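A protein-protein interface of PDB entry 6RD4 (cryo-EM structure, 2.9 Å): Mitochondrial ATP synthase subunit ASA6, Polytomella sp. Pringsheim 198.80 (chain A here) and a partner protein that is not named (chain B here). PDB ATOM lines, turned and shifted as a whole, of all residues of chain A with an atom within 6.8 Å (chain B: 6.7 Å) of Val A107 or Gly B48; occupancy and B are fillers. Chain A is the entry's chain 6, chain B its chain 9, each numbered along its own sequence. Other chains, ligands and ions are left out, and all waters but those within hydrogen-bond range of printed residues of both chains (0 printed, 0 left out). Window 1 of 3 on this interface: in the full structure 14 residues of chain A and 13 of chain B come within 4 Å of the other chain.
A ring nitrogen (ND1) of His B41 is in hydrogen-bond range of the backbone carbonyl oxygen (O) of Ala A111, 3.0 Å away.
Among the printed residues, merely in contact across the chains: Leu A103 with Leu B52, Asn A104 with Gly B48, Asn A104 with Val B49, Asn A104 with Leu B52, Val A107 with Phe B44, Val A107 with Gly B48, Leu A108 with Val B45, Ala A111 with Phe B44, Ala A111 with Val B45 and Trp A112 with His B41.
Of the 12 printed residues of chain B, 6 touch a printed residue of chain A.
Hydrophobic or aromatic side chains of chain B within 4 Å of the printed part of chain A: His B41, Phe B44, Val B45, Val B49 and Leu B52.
Of the 11 printed residues of chain A, 6 touch a printed residue of chain B.
Hydrophobic or aromatic side chains of chain A that line the printed part of chain B: Leu A103, Val A107, Leu A108, Ala A111 and Trp A112.
Among the printed residues, 11 pairs touch across the chains.
Among the printed residues, no Asp or Glu carboxylate lies within 4 Å of a Lys or Arg side-chain nitrogen of the other chain.
Asp A102 touches none of the printed residues of chain B.
Of the printed residues of chain B, Leu A103 touches Leu B52 (3.9 Å).
Printed residues of chain B within 4 Å of Leu A108: Val B45 (3.8 Å).
Of the printed residues of chain A, Val B45 touches Leu A108 (3.8 Å) and Ala A111 (3.9 Å).
Of chain A, only Asn A104 and Val A107 come within 4 Å of Gly B48.
Of the printed residues of chain A, Val B49 touches Asn A104 (3.6 Å).
Val B51 touches none of the printed residues of chain A.
Printed residues of chain A within 4 Å of Leu B52: Leu A103 and Asn A104.
The nearest residue of chain B that does not touch Val A107 is Leu B52 (4.2 Å).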
ATOM      1  N   ASP A 102       6.436 -21.961  11.844  1.00  0.00           N
ATOM      2  CA  ASP A 102       7.396 -21.326  12.739  1.00  0.00           C
ATOM      3  C   ASP A 102       7.068 -19.862  12.947  1.00  0.00           C
ATOM      4  O   ASP A 102       7.149 -19.363  14.066  1.00  0.00           O
ATOM      5  CB  ASP A 102       8.812 -21.437  12.190  1.00  0.00           C
ATOM      6  CG  ASP A 102       9.339 -22.836  12.224  1.00  0.00           C
ATOM      7  OD1 ASP A 102       8.535 -23.751  12.410  1.00  0.00           O
ATOM      8  OD2 ASP A 102      10.558 -23.024  12.061  1.00  0.00           O
ATOM      9  N   LEU A 103       6.693 -19.158  11.888  1.00  0.00           N
ATOM     10  CA  LEU A 103       6.375 -17.749  12.024  1.00  0.00           C
ATOM     11  C   LEU A 103       5.019 -17.521  12.661  1.00  0.00           C
ATOM     12  O   LEU A 103       4.769 -16.429  13.164  1.00  0.00           O
ATOM     13  CB  LEU A 103       6.426 -17.068  10.669  1.00  0.00           C
ATOM     14  CG  LEU A 103       7.813 -16.942  10.063  1.00  0.00           C
ATOM     15  CD1 LEU A 103       7.640 -16.584   8.637  1.00  0.00           C
ATOM     16  CD2 LEU A 103       8.657 -15.926  10.761  1.00  0.00           C
ATOM     17  N   ASN A 104       4.133 -18.502  12.642  1.00  0.00           N
ATOM     18  CA  ASN A 104       2.899 -18.383  13.395  1.00  0.00           C
ATOM     19  C   ASN A 104       3.013 -18.894  14.814  1.00  0.00           C
ATOM     20  O   ASN A 104       2.036 -18.811  15.554  1.00  0.00           O
ATOM     21  CB  ASN A 104       1.748 -19.104  12.702  1.00  0.00           C
ATOM     22  CG  ASN A 104       1.189 -18.313  11.551  1.00  0.00           C
ATOM     23  OD1 ASN A 104       1.196 -18.748  10.410  1.00  0.00           O
ATOM     24  ND2 ASN A 104       0.707 -17.123  11.851  1.00  0.00           N
ATOM     25  N   LEU A 105       4.150 -19.445  15.208  1.00  0.00           N
ATOM     26  CA  LEU A 105       4.351 -19.702  16.622  1.00  0.00           C
ATOM     27  C   LEU A 105       4.868 -18.493  17.360  1.00  0.00           C
ATOM     28  O   LEU A 105       4.583 -18.362  18.544  1.00  0.00           O
ATOM     29  CB  LEU A 105       5.294 -20.869  16.844  1.00  0.00           C
ATOM     30  CG  LEU A 105       4.622 -22.208  16.628  1.00  0.00           C
ATOM     31  CD1 LEU A 105       5.590 -23.276  16.908  1.00  0.00           C
ATOM     32  CD2 LEU A 105       3.475 -22.338  17.554  1.00  0.00           C
ATOM     33  N   ASN A 106       5.598 -17.604  16.697  1.00  0.00           N
ATOM     34  CA  ASN A 106       5.970 -16.350  17.327  1.00  0.00           C
ATOM     35  C   ASN A 106       4.768 -15.465  17.584  1.00  0.00           C
ATOM     36  O   ASN A 106       4.819 -14.621  18.471  1.00  0.00           O
ATOM     37  CB  ASN A 106       6.972 -15.603  16.470  1.00  0.00           C
ATOM     38  CG  ASN A 106       8.041 -16.493  15.937  1.00  0.00           C
ATOM     39  OD1 ASN A 106       8.378 -17.497  16.538  1.00  0.00           O
ATOM     40  ND2 ASN A 106       8.592 -16.129  14.805  1.00  0.00           N
ATOM     41  N   VAL A 107       3.693 -15.628  16.824  1.00  0.00           N
ATOM     42  CA  VAL A 107       2.459 -14.915  17.116  1.00  0.00           C
ATOM     43  C   VAL A 107       1.758 -15.542  18.307  1.00  0.00           C
ATOM     44  O   VAL A 107       1.164 -14.845  19.129  1.00  0.00           O
ATOM     45  CB  VAL A 107       1.574 -14.903  15.859  1.00  0.00           C
ATOM     46  CG1 VAL A 107       0.282 -14.207  16.109  1.00  0.00           C
ATOM     47  CG2 VAL A 107       2.296 -14.228  14.749  1.00  0.00           C
ATOM     48  N   LEU A 108       1.846 -16.859  18.443  1.00  0.00           N
ATOM     49  CA  LEU A 108       1.251 -17.523  19.592  1.00  0.00           C
ATOM     50  C   LEU A 108       2.036 -17.266  20.857  1.00  0.00           C
ATOM     51  O   LEU A 108       1.456 -17.202  21.939  1.00  0.00           O
ATOM     52  CB  LEU A 108       1.180 -19.016  19.352  1.00  0.00           C
ATOM     53  CG  LEU A 108      -0.072 -19.539  18.703  1.00  0.00           C
ATOM     54  CD1 LEU A 108       0.113 -20.992  18.503  1.00  0.00           C
ATOM     55  CD2 LEU A 108      -1.184 -19.296  19.644  1.00  0.00           C
ATOM     56  N   GLN A 109       3.348 -17.148  20.746  1.00  0.00           N
ATOM     57  CA  GLN A 109       4.169 -16.920  21.916  1.00  0.00           C
ATOM     58  C   GLN A 109       4.115 -15.477  22.369  1.00  0.00           C
ATOM     59  O   GLN A 109       4.129 -15.219  23.570  1.00  0.00           O
ATOM     60  CB  GLN A 109       5.601 -17.325  21.623  1.00  0.00           C
ATOM     61  CG  GLN A 109       5.782 -18.785  21.549  1.00  0.00           C
ATOM     62  CD  GLN A 109       7.046 -19.150  20.861  1.00  0.00           C
ATOM     63  OE1 GLN A 109       7.724 -18.307  20.311  1.00  0.00           O
ATOM     64  NE2 GLN A 109       7.383 -20.420  20.892  1.00  0.00           N
ATOM     65  N   ALA A 110       4.053 -14.529  21.438  1.00  0.00           N
ATOM     66  CA  ALA A 110       3.927 -13.129  21.799  1.00  0.00           C
ATOM     67  C   ALA A 110       2.526 -12.749  22.210  1.00  0.00           C
ATOM     68  O   ALA A 110       2.322 -11.633  22.675  1.00  0.00           O
ATOM     69  CB  ALA A 110       4.345 -12.225  20.652  1.00  0.00           C
ATOM     70  N   ALA A 111       1.552 -13.623  22.020  1.00  0.00           N
ATOM     71  CA  ALA A 111       0.215 -13.324  22.496  1.00  0.00           C
ATOM     72  C   ALA A 111       0.137 -13.480  23.998  1.00  0.00           C
ATOM     73  O   ALA A 111      -0.703 -12.854  24.645  1.00  0.00           O
ATOM     74  CB  ALA A 111      -0.799 -14.228  21.818  1.00  0.00           C
ATOM     75  N   TRP A 112       0.986 -14.327  24.570  1.00  0.00           N
ATOM     76  CA  TRP A 112       1.016 -14.522  26.009  1.00  0.00           C
ATOM     77  C   TRP A 112       1.869 -13.497  26.715  1.00  0.00           C
ATOM     78  O   TRP A 112       1.647 -13.240  27.893  1.00  0.00           O
ATOM     79  CB  TRP A 112       1.530 -15.907  26.341  1.00  0.00           C
ATOM     80  CG  TRP A 112       0.478 -16.891  26.373  1.00  0.00           C
ATOM     81  CD1 TRP A 112       0.168 -17.763  25.404  1.00  0.00           C
ATOM     82  CD2 TRP A 112      -0.446 -17.111  27.425  1.00  0.00           C
ATOM     83  NE1 TRP A 112      -0.892 -18.529  25.777  1.00  0.00           N
ATOM     84  CE2 TRP A 112      -1.289 -18.142  27.024  1.00  0.00           C
ATOM     85  CE3 TRP A 112      -0.646 -16.528  28.668  1.00  0.00           C
ATOM     86  CZ2 TRP A 112      -2.316 -18.610  27.817  1.00  0.00           C
ATOM     87  CZ3 TRP A 112      -1.659 -16.994  29.455  1.00  0.00           C
ATOM     88  CH2 TRP A 112      -2.481 -18.027  29.032  1.00  0.00           C
ATOM     89  N   HIS B  41      -6.755 -11.867  23.411  1.00  0.00           N
ATOM     90  CA  HIS B  41      -5.685 -12.830  23.197  1.00  0.00           C
ATOM     91  C   HIS B  41      -5.963 -13.701  21.987  1.00  0.00           C
ATOM     92  O   HIS B  41      -5.137 -13.795  21.078  1.00  0.00           O
ATOM     93  CB  HIS B  41      -5.526 -13.685  24.446  1.00  0.00           C
ATOM     94  CG  HIS B  41      -4.432 -14.691  24.356  1.00  0.00           C
ATOM     95  ND1 HIS B  41      -3.173 -14.465  24.853  1.00  0.00           N
ATOM     96  CD2 HIS B  41      -4.415 -15.937  23.841  1.00  0.00           C
ATOM     97  CE1 HIS B  41      -2.422 -15.524  24.634  1.00  0.00           C
ATOM     98  NE2 HIS B  41      -3.152 -16.430  24.018  1.00  0.00           N
ATOM     99  N   GLY B  43      -8.171 -13.105  19.781  1.00  0.00           N
ATOM    100  CA  GLY B  43      -8.292 -12.209  18.650  1.00  0.00           C
ATOM    101  C   GLY B  43      -6.952 -11.818  18.066  1.00  0.00           C
ATOM    102  O   GLY B  43      -6.836 -11.613  16.864  1.00  0.00           O
ATOM    103  N   PHE B  44      -5.927 -11.704  18.905  1.00  0.00           N
ATOM    104  CA  PHE B  44      -4.587 -11.406  18.410  1.00  0.00           C
ATOM    105  C   PHE B  44      -4.026 -12.568  17.609  1.00  0.00           C
ATOM    106  O   PHE B  44      -3.267 -12.356  16.663  1.00  0.00           O
ATOM    107  CB  PHE B  44      -3.668 -11.082  19.589  1.00  0.00           C
ATOM    108  CG  PHE B  44      -2.252 -10.759  19.210  1.00  0.00           C
ATOM    109  CD1 PHE B  44      -1.897  -9.492  18.829  1.00  0.00           C
ATOM    110  CD2 PHE B  44      -1.268 -11.719  19.277  1.00  0.00           C
ATOM    111  CE1 PHE B  44      -0.596  -9.200  18.503  1.00  0.00           C
ATOM    112  CE2 PHE B  44       0.019 -11.430  18.940  1.00  0.00           C
ATOM    113  CZ  PHE B  44       0.355 -10.173  18.557  1.00  0.00           C
ATOM    114  N   VAL B  45      -4.382 -13.794  17.983  1.00  0.00           N
ATOM    115  CA  VAL B  45      -3.885 -14.961  17.272  1.00  0.00           C
ATOM    116  C   VAL B  45      -4.580 -15.096  15.925  1.00  0.00           C
ATOM    117  O   VAL B  45      -3.927 -15.332  14.904  1.00  0.00           O
ATOM    118  CB  VAL B  45      -4.059 -16.214  18.145  1.00  0.00           C
ATOM    119  CG1 VAL B  45      -3.653 -17.439  17.401  1.00  0.00           C
ATOM    120  CG2 VAL B  45      -3.237 -16.090  19.381  1.00  0.00           C
ATOM    121  N   MET B  46      -5.904 -14.916  15.892  1.00  0.00           N
ATOM    122  CA  MET B  46      -6.650 -15.057  14.644  1.00  0.00           C
ATOM    123  C   MET B  46      -6.303 -13.956  13.661  1.00  0.00           C
ATOM    124  O   MET B  46      -6.281 -14.187  12.453  1.00  0.00           O
ATOM    125  CB  MET B  46      -8.144 -15.037  14.913  1.00  0.00           C
ATOM    126  CG  MET B  46      -8.670 -16.208  15.674  1.00  0.00           C
ATOM    127  SD  MET B  46     -10.461 -16.272  15.590  1.00  0.00           S
ATOM    128  CE  MET B  46     -10.885 -14.574  15.954  1.00  0.00           C
ATOM    129  N   VAL B  47      -6.045 -12.751  14.156  1.00  0.00           N
ATOM    130  CA  VAL B  47      -5.580 -11.686  13.279  1.00  0.00           C
ATOM    131  C   VAL B  47      -4.168 -11.972  12.803  1.00  0.00           C
ATOM    132  O   VAL B  47      -3.854 -11.800  11.624  1.00  0.00           O
ATOM    133  CB  VAL B  47      -5.691 -10.329  13.992  1.00  0.00           C
ATOM    134  CG1 VAL B  47      -4.976  -9.253  13.228  1.00  0.00           C
ATOM    135  CG2 VAL B  47      -7.136  -9.942  14.110  1.00  0.00           C
ATOM    136  N   GLY B  48      -3.310 -12.466  13.690  1.00  0.00           N
ATOM    137  CA  GLY B  48      -1.933 -12.722  13.309  1.00  0.00           C
ATOM    138  C   GLY B  48      -1.773 -13.924  12.411  1.00  0.00           C
ATOM    139  O   GLY B  48      -0.838 -13.981  11.615  1.00  0.00           O
ATOM    140  N   VAL B  49      -2.659 -14.905  12.537  1.00  0.00           N
ATOM    141  CA  VAL B  49      -2.674 -16.015  11.592  1.00  0.00           C
ATOM    142  C   VAL B  49      -3.139 -15.544  10.220  1.00  0.00           C
ATOM    143  O   VAL B  49      -2.513 -15.849   9.201  1.00  0.00           O
ATOM    144  CB  VAL B  49      -3.552 -17.150  12.146  1.00  0.00           C
ATOM    145  CG1 VAL B  49      -4.023 -18.063  11.055  1.00  0.00           C
ATOM    146  CG2 VAL B  49      -2.773 -17.934  13.170  1.00  0.00           C
ATOM    147  N   ASN B  50      -4.210 -14.752  10.177  1.00  0.00           N
ATOM    148  CA  ASN B  50      -4.759 -14.293   8.911  1.00  0.00           C
ATOM    149  C   ASN B  50      -3.877 -13.256   8.234  1.00  0.00           C
ATOM    150  O   ASN B  50      -3.992 -13.059   7.026  1.00  0.00           O
ATOM    151  CB  ASN B  50      -6.154 -13.731   9.131  1.00  0.00           C
ATOM    152  CG  ASN B  50      -7.164 -14.805   9.447  1.00  0.00           C
ATOM    153  OD1 ASN B  50      -7.206 -15.837   8.791  1.00  0.00           O
ATOM    154  ND2 ASN B  50      -7.978 -14.575  10.461  1.00  0.00           N
ATOM    155  N   VAL B  51      -3.016 -12.565   8.974  1.00  0.00           N
ATOM    156  CA  VAL B  51      -2.064 -11.666   8.332  1.00  0.00           C
ATOM    157  C   VAL B  51      -0.891 -12.444   7.765  1.00  0.00           C
ATOM    158  O   VAL B  51      -0.445 -12.176   6.647  1.00  0.00           O
ATOM    159  CB  VAL B  51      -1.613 -10.575   9.318  1.00  0.00           C
ATOM    160  CG1 VAL B  51      -0.415  -9.814   8.798  1.00  0.00           C
ATOM    161  CG2 VAL B  51      -2.728  -9.599   9.534  1.00  0.00           C
ATOM    162  N   LEU B  52      -0.388 -13.433   8.505  1.00  0.00           N
ATOM    163  CA  LEU B  52       0.767 -14.204   8.051  1.00  0.00           C
ATOM    164  C   LEU B  52       0.442 -15.049   6.834  1.00  0.00           C
ATOM    165  O   LEU B  52       1.301 -15.237   5.973  1.00  0.00           O
ATOM    166  CB  LEU B  52       1.287 -15.104   9.168  1.00  0.00           C
ATOM    167  CG  LEU B  52       2.474 -14.674  10.025  1.00  0.00           C
ATOM    168  CD1 LEU B  52       3.708 -14.646   9.174  1.00  0.00           C
ATOM    169  CD2 LEU B  52       2.257 -13.329  10.662  1.00  0.00           C
ATOM    170  N   LEU B  53      -0.786 -15.544   6.735  1.00  0.00           N
ATOM    171  CA  LEU B  53      -1.177 -16.292   5.552  1.00  0.00           C
ATOM    172  C   LEU B  53      -1.363 -15.369   4.360  1.00  0.00           C
ATOM    173  O   LEU B  53      -0.838 -15.631   3.276  1.00  0.00           O
ATOM    174  CB  LEU B  53      -2.459 -17.066   5.825  1.00  0.00           C
ATOM    175  CG  LEU B  53      -2.291 -18.368   6.588  1.00  0.00           C
ATOM    176  CD1 LEU B  53      -3.603 -19.077   6.708  1.00  0.00           C
ATOM    177  CD2 LEU B  53      -1.313 -19.234   5.876  1.00  0.00           C
